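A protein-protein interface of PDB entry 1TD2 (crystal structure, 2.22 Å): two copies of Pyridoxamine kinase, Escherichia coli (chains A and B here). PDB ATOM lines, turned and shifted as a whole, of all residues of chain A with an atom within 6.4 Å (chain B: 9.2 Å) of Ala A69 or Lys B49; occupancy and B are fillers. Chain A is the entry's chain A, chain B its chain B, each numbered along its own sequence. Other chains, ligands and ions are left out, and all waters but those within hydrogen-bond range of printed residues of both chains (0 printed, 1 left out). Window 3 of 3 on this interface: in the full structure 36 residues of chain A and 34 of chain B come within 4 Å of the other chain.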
ATOM      1  N   VAL A  64      25.395  -3.999  -1.943  1.00  0.00           N
ATOM      2  CA  VAL A  64      25.221  -2.890  -2.868  1.00  0.00           C
ATOM      3  C   VAL A  64      24.199  -1.865  -2.343  1.00  0.00           C
ATOM      4  O   VAL A  64      24.389  -0.651  -2.530  1.00  0.00           O
ATOM      5  CB  VAL A  64      24.888  -3.448  -4.269  1.00  0.00           C
ATOM      6  CG1 VAL A  64      24.575  -2.321  -5.269  1.00  0.00           C
ATOM      7  CG2 VAL A  64      26.086  -4.285  -4.731  1.00  0.00           C
ATOM      8  N   GLN A  65      23.137  -2.344  -1.682  1.00  0.00           N
ATOM      9  CA  GLN A  65      22.151  -1.450  -1.068  1.00  0.00           C
ATOM     10  C   GLN A  65      22.929  -0.563  -0.099  1.00  0.00           C
ATOM     11  O   GLN A  65      22.632   0.617   0.082  1.00  0.00           O
ATOM     12  CB  GLN A  65      21.119  -2.260  -0.275  1.00  0.00           C
ATOM     13  CG  GLN A  65      20.049  -2.874  -1.137  1.00  0.00           C
ATOM     14  CD  GLN A  65      19.182  -1.793  -1.772  1.00  0.00           C
ATOM     15  OE1 GLN A  65      19.693  -0.815  -2.332  1.00  0.00           O
ATOM     16  NE2 GLN A  65      17.866  -1.960  -1.685  1.00  0.00           N
ATOM     17  N   GLY A  66      23.940  -1.150   0.531  1.00  0.00           N
ATOM     18  CA  GLY A  66      24.740  -0.395   1.475  1.00  0.00           C
ATOM     19  C   GLY A  66      25.495   0.743   0.803  1.00  0.00           C
ATOM     20  O   GLY A  66      25.523   1.871   1.311  1.00  0.00           O
ATOM     21  N   ILE A  67      26.099   0.455  -0.348  1.00  0.00           N
ATOM     22  CA  ILE A  67      26.867   1.455  -1.058  1.00  0.00           C
ATOM     23  C   ILE A  67      25.921   2.537  -1.580  1.00  0.00           C
ATOM     24  O   ILE A  67      26.286   3.722  -1.625  1.00  0.00           O
ATOM     25  CB  ILE A  67      27.669   0.824  -2.207  1.00  0.00           C
ATOM     26  CG1 ILE A  67      28.458  -0.378  -1.691  1.00  0.00           C
ATOM     27  CG2 ILE A  67      28.654   1.844  -2.763  1.00  0.00           C
ATOM     28  CD1 ILE A  67      29.169  -1.162  -2.793  1.00  0.00           C
ATOM     29  N   ALA A  68      24.708   2.131  -1.963  1.00  0.00           N
ATOM     30  CA  ALA A  68      23.689   3.089  -2.425  1.00  0.00           C
ATOM     31  C   ALA A  68      23.333   4.035  -1.259  1.00  0.00           C
ATOM     32  O   ALA A  68      23.281   5.254  -1.422  1.00  0.00           O
ATOM     33  CB  ALA A  68      22.414   2.340  -2.893  1.00  0.00           C
ATOM     34  N   ALA A  69      23.096   3.443  -0.091  1.00  0.00           N
ATOM     35  CA  ALA A  69      22.765   4.164   1.129  1.00  0.00           C
ATOM     36  C   ALA A  69      23.711   5.318   1.425  1.00  0.00           C
ATOM     37  O   ALA A  69      23.270   6.386   1.878  1.00  0.00           O
ATOM     38  CB  ALA A  69      22.738   3.198   2.307  1.00  0.00           C
ATOM     39  N   ILE A  70      25.004   5.129   1.178  1.00  0.00           N
ATOM     40  CA  ILE A  70      25.944   6.222   1.425  1.00  0.00           C
ATOM     41  C   ILE A  70      26.154   7.085   0.189  1.00  0.00           C
ATOM     42  O   ILE A  70      27.039   7.937   0.156  1.00  0.00           O
ATOM     43  CB  ILE A  70      27.324   5.727   1.969  1.00  0.00           C
ATOM     44  CG1 ILE A  70      27.903   4.616   1.086  1.00  0.00           C
ATOM     45  CG2 ILE A  70      27.161   5.270   3.393  1.00  0.00           C
ATOM     46  CD1 ILE A  70      29.323   4.201   1.480  1.00  0.00           C
ATOM     47  N   ASP A  71      25.316   6.862  -0.821  1.00  0.00           N
ATOM     48  CA  ASP A  71      25.362   7.631  -2.053  1.00  0.00           C
ATOM     49  C   ASP A  71      26.648   7.498  -2.817  1.00  0.00           C
ATOM     50  O   ASP A  71      27.182   8.490  -3.285  1.00  0.00           O
ATOM     51  CB  ASP A  71      25.128   9.118  -1.773  1.00  0.00           C
ATOM     52  CG  ASP A  71      23.901   9.353  -0.947  1.00  0.00           C
ATOM     53  OD1 ASP A  71      22.826   8.848  -1.337  1.00  0.00           O
ATOM     54  OD2 ASP A  71      24.012  10.038   0.094  1.00  0.00           O
ATOM     55  N   LYS A  72      27.141   6.279  -2.977  1.00  0.00           N
ATOM     56  CA  LYS A  72      28.388   6.128  -3.696  1.00  0.00           C
ATOM     57  C   LYS A  72      28.278   5.333  -4.975  1.00  0.00           C
ATOM     58  O   LYS A  72      29.183   5.373  -5.814  1.00  0.00           O
ATOM     59  CB  LYS A  72      29.434   5.526  -2.762  1.00  0.00           C
ATOM     60  CG  LYS A  72      29.794   6.496  -1.666  1.00  0.00           C
ATOM     61  CD  LYS A  72      30.300   7.792  -2.288  1.00  0.00           C
ATOM     62  CE  LYS A  72      30.803   8.750  -1.221  1.00  0.00           C
ATOM     63  NZ  LYS A  72      31.322  10.023  -1.806  1.00  0.00           N
ATOM     64  N   GLN A  99      21.012  -1.699 -10.966  1.00  0.00           N
ATOM     65  CA  GLN A  99      21.037  -0.680  -9.936  1.00  0.00           C
ATOM     66  C   GLN A  99      22.185   0.283 -10.178  1.00  0.00           C
ATOM     67  O   GLN A  99      22.007   1.499 -10.068  1.00  0.00           O
ATOM     68  CB  GLN A  99      21.161  -1.299  -8.542  1.00  0.00           C
ATOM     69  CG  GLN A  99      20.729  -0.326  -7.449  1.00  0.00           C
ATOM     70  CD  GLN A  99      20.908  -0.868  -6.035  1.00  0.00           C
ATOM     71  OE1 GLN A  99      20.777  -2.066  -5.788  1.00  0.00           O
ATOM     72  NE2 GLN A  99      21.185   0.028  -5.093  1.00  0.00           N
ATOM     73  N   VAL B  12      35.923  -4.176   3.838  1.00  0.00           N
ATOM     74  CA  VAL B  12      34.801  -3.365   3.368  1.00  0.00           C
ATOM     75  C   VAL B  12      34.855  -3.410   1.848  1.00  0.00           C
ATOM     76  O   VAL B  12      35.944  -3.317   1.261  1.00  0.00           O
ATOM     77  CB  VAL B  12      34.901  -1.900   3.823  1.00  0.00           C
ATOM     78  CG1 VAL B  12      34.431  -1.799   5.272  1.00  0.00           C
ATOM     79  CG2 VAL B  12      36.352  -1.390   3.673  1.00  0.00           C
ATOM     80  N   TYR B  14      33.230  -1.207  -0.305  1.00  0.00           N
ATOM     81  CA  TYR B  14      33.518   0.168  -0.721  1.00  0.00           C
ATOM     82  C   TYR B  14      34.483   0.782   0.307  1.00  0.00           C
ATOM     83  O   TYR B  14      34.368   0.509   1.503  1.00  0.00           O
ATOM     84  CB  TYR B  14      32.255   1.028  -0.740  1.00  0.00           C
ATOM     85  CG  TYR B  14      32.526   2.475  -1.097  1.00  0.00           C
ATOM     86  CD1 TYR B  14      32.902   3.415  -0.123  1.00  0.00           C
ATOM     87  CD2 TYR B  14      32.472   2.893  -2.423  1.00  0.00           C
ATOM     88  CE1 TYR B  14      33.219   4.732  -0.478  1.00  0.00           C
ATOM     89  CE2 TYR B  14      32.792   4.195  -2.779  1.00  0.00           C
ATOM     90  CZ  TYR B  14      33.166   5.105  -1.815  1.00  0.00           C
ATOM     91  OH  TYR B  14      33.558   6.359  -2.231  1.00  0.00           O
ATOM     92  N   PHE B  41      31.620  -6.006   5.053  1.00  0.00           N
ATOM     93  CA  PHE B  41      30.695  -4.883   5.165  1.00  0.00           C
ATOM     94  C   PHE B  41      30.666  -4.045   3.886  1.00  0.00           C
ATOM     95  O   PHE B  41      31.641  -3.995   3.137  1.00  0.00           O
ATOM     96  CB  PHE B  41      31.104  -3.988   6.333  1.00  0.00           C
ATOM     97  CG  PHE B  41      30.946  -4.634   7.691  1.00  0.00           C
ATOM     98  CD1 PHE B  41      31.478  -4.018   8.828  1.00  0.00           C
ATOM     99  CD2 PHE B  41      30.256  -5.837   7.840  1.00  0.00           C
ATOM    100  CE1 PHE B  41      31.322  -4.587  10.095  1.00  0.00           C
ATOM    101  CE2 PHE B  41      30.093  -6.421   9.111  1.00  0.00           C
ATOM    102  CZ  PHE B  41      30.625  -5.792  10.233  1.00  0.00           C
ATOM    103  N   SER B  42      29.552  -3.369   3.643  1.00  0.00           N
ATOM    104  CA  SER B  42      29.453  -2.539   2.449  1.00  0.00           C
ATOM    105  C   SER B  42      30.446  -1.377   2.505  1.00  0.00           C
ATOM    106  O   SER B  42      30.991  -0.971   1.483  1.00  0.00           O
ATOM    107  CB  SER B  42      28.019  -2.005   2.271  1.00  0.00           C
ATOM    108  OG  SER B  42      27.564  -1.314   3.425  1.00  0.00           O
ATOM    109  N   ASN B  43      30.689  -0.854   3.703  1.00  0.00           N
ATOM    110  CA  ASN B  43      31.599   0.281   3.880  1.00  0.00           C
ATOM    111  C   ASN B  43      31.964   0.252   5.348  1.00  0.00           C
ATOM    112  O   ASN B  43      31.446  -0.589   6.081  1.00  0.00           O
ATOM    113  CB  ASN B  43      30.855   1.578   3.585  1.00  0.00           C
ATOM    114  CG  ASN B  43      29.557   1.655   4.353  1.00  0.00           C
ATOM    115  OD1 ASN B  43      28.521   1.155   3.903  1.00  0.00           O
ATOM    116  ND2 ASN B  43      29.619   2.220   5.551  1.00  0.00           N
ATOM    117  N   HIS B  44      32.817   1.169   5.803  1.00  0.00           N
ATOM    118  CA  HIS B  44      33.194   1.147   7.213  1.00  0.00           C
ATOM    119  C   HIS B  44      32.134   1.803   8.137  1.00  0.00           C
ATOM    120  O   HIS B  44      31.233   2.515   7.665  1.00  0.00           O
ATOM    121  CB  HIS B  44      34.589   1.765   7.418  1.00  0.00           C
ATOM    122  CG  HIS B  44      34.648   3.249   7.229  1.00  0.00           C
ATOM    123  ND1 HIS B  44      35.483   3.848   6.309  1.00  0.00           N
ATOM    124  CD2 HIS B  44      34.003   4.257   7.867  1.00  0.00           C
ATOM    125  CE1 HIS B  44      35.348   5.162   6.384  1.00  0.00           C
ATOM    126  NE2 HIS B  44      34.456   5.437   7.322  1.00  0.00           N
ATOM    127  N   THR B  45      32.245   1.547   9.443  1.00  0.00           N
ATOM    128  CA  THR B  45      31.285   2.060  10.439  1.00  0.00           C
ATOM    129  C   THR B  45      31.228   3.562  10.730  1.00  0.00           C
ATOM    130  O   THR B  45      30.248   4.025  11.296  1.00  0.00           O
ATOM    131  CB  THR B  45      31.446   1.379  11.816  1.00  0.00           C
ATOM    132  OG1 THR B  45      32.703   1.759  12.402  1.00  0.00           O
ATOM    133  CG2 THR B  45      31.348  -0.129  11.681  1.00  0.00           C
ATOM    134  N   GLN B  46      32.250   4.325  10.349  1.00  0.00           N
ATOM    135  CA  GLN B  46      32.217   5.755  10.622  1.00  0.00           C
ATOM    136  C   GLN B  46      31.124   6.447   9.792  1.00  0.00           C
ATOM    137  O   GLN B  46      30.763   7.586  10.073  1.00  0.00           O
ATOM    138  CB  GLN B  46      33.591   6.402  10.358  1.00  0.00           C
ATOM    139  CG  GLN B  46      33.776   7.763  11.046  1.00  0.00           C
ATOM    140  CD  GLN B  46      35.110   8.445  10.729  1.00  0.00           C
ATOM    141  OE1 GLN B  46      35.315   8.975   9.638  1.00  0.00           O
ATOM    142  NE2 GLN B  46      36.020   8.428  11.694  1.00  0.00           N
ATOM    143  N   TYR B  47      30.579   5.757   8.793  1.00  0.00           N
ATOM    144  CA  TYR B  47      29.515   6.343   7.960  1.00  0.00           C
ATOM    145  C   TYR B  47      28.215   6.416   8.744  1.00  0.00           C
ATOM    146  O   TYR B  47      27.290   7.146   8.371  1.00  0.00           O
ATOM    147  CB  TYR B  47      29.264   5.520   6.686  1.00  0.00           C
ATOM    148  CG  TYR B  47      30.298   5.731   5.597  1.00  0.00           C
ATOM    149  CD1 TYR B  47      31.449   4.946   5.534  1.00  0.00           C
ATOM    150  CD2 TYR B  47      30.129   6.719   4.633  1.00  0.00           C
ATOM    151  CE1 TYR B  47      32.401   5.136   4.531  1.00  0.00           C
ATOM    152  CE2 TYR B  47      31.072   6.918   3.634  1.00  0.00           C
ATOM    153  CZ  TYR B  47      32.208   6.117   3.589  1.00  0.00           C
ATOM    154  OH  TYR B  47      33.139   6.311   2.587  1.00  0.00           O
ATOM    155  N   GLY B  48      28.151   5.649   9.825  1.00  0.00           N
ATOM    156  CA  GLY B  48      26.950   5.629  10.639  1.00  0.00           C
ATOM    157  C   GLY B  48      25.951   4.589  10.148  1.00  0.00           C
ATOM    158  O   GLY B  48      24.842   4.495  10.673  1.00  0.00           O
ATOM    159  N   LYS B  49      26.338   3.813   9.136  1.00  0.00           N
ATOM    160  CA  LYS B  49      25.470   2.783   8.577  1.00  0.00           C
ATOM    161  C   LYS B  49      26.254   1.900   7.617  1.00  0.00           C
ATOM    162  O   LYS B  49      27.210   2.354   6.996  1.00  0.00           O
ATOM    163  CB  LYS B  49      24.304   3.422   7.836  1.00  0.00           C
ATOM    164  CG  LYS B  49      24.731   4.416   6.761  1.00  0.00           C
ATOM    165  CD  LYS B  49      23.518   4.911   6.006  1.00  0.00           C
ATOM    166  CE  LYS B  49      23.771   6.255   5.347  1.00  0.00           C
ATOM    167  NZ  LYS B  49      22.470   6.975   5.227  1.00  0.00           N
ATOM    168  N   TRP B  50      25.823   0.653   7.465  1.00  0.00           N
ATOM    169  CA  TRP B  50      26.530  -0.280   6.610  1.00  0.00           C
ATOM    170  C   TRP B  50      25.812  -1.619   6.616  1.00  0.00           C
ATOM    171  O   TRP B  50      25.166  -1.993   7.590  1.00  0.00           O
ATOM    172  CB  TRP B  50      27.980  -0.449   7.111  1.00  0.00           C
ATOM    173  CG  TRP B  50      28.111  -1.128   8.461  1.00  0.00           C
ATOM    174  CD1 TRP B  50      28.304  -2.460   8.690  1.00  0.00           C
ATOM    175  CD2 TRP B  50      28.038  -0.509   9.757  1.00  0.00           C
ATOM    176  NE1 TRP B  50      28.357  -2.711  10.041  1.00  0.00           N
ATOM    177  CE2 TRP B  50      28.196  -1.533  10.718  1.00  0.00           C
ATOM    178  CE3 TRP B  50      27.850   0.812  10.200  1.00  0.00           C
ATOM    179  CZ2 TRP B  50      28.170  -1.280  12.101  1.00  0.00           C
ATOM    180  CZ3 TRP B  50      27.826   1.065  11.573  1.00  0.00           C
ATOM    181  CH2 TRP B  50      27.985   0.021  12.506  1.00  0.00           C
ATOM    182  N   THR B  51      25.915  -2.336   5.513  1.00  0.00           N
ATOM    183  CA  THR B  51      25.271  -3.616   5.415  1.00  0.00           C
ATOM    184  C   THR B  51      26.363  -4.672   5.446  1.00  0.00           C
ATOM    185  O   THR B  51      27.533  -4.330   5.579  1.00  0.00           O
ATOM    186  CB  THR B  51      24.483  -3.694   4.126  1.00  0.00           C
ATOM    187  OG1 THR B  51      25.344  -3.401   3.027  1.00  0.00           O
ATOM    188  CG2 THR B  51      23.333  -2.686   4.147  1.00  0.00           C
ATOM    189  N   GLY B  52      25.994  -5.946   5.328  1.00  0.00           N
ATOM    190  CA  GLY B  52      26.998  -6.996   5.354  1.00  0.00           C
ATOM    191  C   GLY B  52      26.843  -7.931   6.539  1.00  0.00           C
ATOM    192  O   GLY B  52      25.842  -7.891   7.242  1.00  0.00           O
ATOM    193  N   GLY B 121      34.178   7.518  15.808  1.00  0.00           N
ATOM    194  CA  GLY B 121      33.395   6.851  14.780  1.00  0.00           C
ATOM    195  C   GLY B 121      33.610   5.361  14.557  1.00  0.00           C
ATOM    196  O   GLY B 121      32.991   4.788  13.654  1.00  0.00           O
ATOM    197  N   ILE B 123      32.926   1.662  15.398  1.00  0.00           N
ATOM    198  CA  ILE B 123      32.025   0.826  16.176  1.00  0.00           C
ATOM    199  C   ILE B 123      32.527  -0.618  16.214  1.00  0.00           C
ATOM    200  O   ILE B 123      32.655  -1.279  15.180  1.00  0.00           O
ATOM    201  CB  ILE B 123      30.597   0.882  15.608  1.00  0.00           C
ATOM    202  CG1 ILE B 123      30.093   2.325  15.652  1.00  0.00           C
ATOM    203  CG2 ILE B 123      29.669   0.009  16.431  1.00  0.00           C
ATOM    204  CD1 ILE B 123      28.769   2.552  14.967  1.00  0.00           C
ATOM    205  N   TYR B 264      37.437  11.450   1.576  1.00  0.00           N
ATOM    206  CA  TYR B 264      37.178  11.019   2.934  1.00  0.00           C
ATOM    207  C   TYR B 264      37.821   9.640   3.126  1.00  0.00           C
ATOM    208  O   TYR B 264      38.320   9.319   4.198  1.00  0.00           O
ATOM    209  CB  TYR B 264      35.661  10.963   3.138  1.00  0.00           C
ATOM    210  CG  TYR B 264      35.186  10.231   4.364  1.00  0.00           C
ATOM    211  CD1 TYR B 264      35.668  10.560   5.636  1.00  0.00           C
ATOM    212  CD2 TYR B 264      34.203   9.248   4.265  1.00  0.00           C
ATOM    213  CE1 TYR B 264      35.171   9.929   6.785  1.00  0.00           C
ATOM    214  CE2 TYR B 264      33.698   8.611   5.405  1.00  0.00           C
ATOM    215  CZ  TYR B 264      34.180   8.959   6.656  1.00  0.00           C
ATOM    216  OH  TYR B 264      33.638   8.371   7.776  1.00  0.00           O
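The backbone carbonyl oxygen (O) of Ala A69 lies within hydrogen-bond range of the side-chain amino group (NZ) of Lys B49, at 3.5 Å.
The backbone NH (N) of Lys A72 lies within hydrogen-bond range of the backbone carbonyl oxygen (O) of Ile A67.
The backbone NH (N) of Tyr B14 lies within hydrogen-bond range of the backbone carbonyl oxygen (O) of Ser B42, 2.9 Å away.
The side-chain hydroxyl (OG) of Ser B42 is in hydrogen-bond range of the side-chain amide oxygen (OD1) of Asn B43 (2.7 Å).
The side-chain hydroxyl (OG) of Ser B42 is in hydrogen-bond range of the backbone NH (N) of Thr B51 (2.9 Å).
The side-chain amide nitrogen of Asn B43 is in hydrogen-bond range of the backbone carbonyl oxygen of Lys B49 (2.8 Å).
CA of Gly A66 touches OG of Ser B42 (3.6 Å).
CA of Gly A66 touches OG1 of Thr B51 (3.4 Å).
Ile A67 touches Tyr B14.
CD1 of Tyr B14 touches CD1 of Ile A70, at 3.9996 Å.
CB of Asn B43 touches CD1 of Ile A70 (3.7 Å).
Tyr B47 touches Ile A70.
Lys A72 touches Tyr B14.
Of chain B, only Lys B49 comes within 4 Å of Ala A69.
Of the printed residues of chain A, Lys B49 touches Ala A69 (3.5 Å).
Gly A66 touches two residues of chain B.
No residue of chain B comes within 4 Å of Ala A68.
Of the printed residues of chain A, Asn B43 touches Ile A70 (3.7 Å).
Of the printed residues of chain A, Tyr B47 touches Ile A70.
Val B12 touches none of the printed residues of chain A.
Printed residues of chain B that touch a printed residue of chain A: Tyr B14, Ser B42, Asn B43, Tyr B47, Lys B49 and Thr B51.
Hydrophobic or aromatic side chains of chain B that line the printed part of chain A: Tyr B14 and Tyr B47.
Hydrophobic or aromatic side chains of chain A that line the printed part of chain B: Ile A67 and Ile A70.
Among the printed residues, no Asp or Glu carboxylate lies within 4 Å of a Lys or Arg side-chain nitrogen of the other chain.
No position is printed for both chains.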
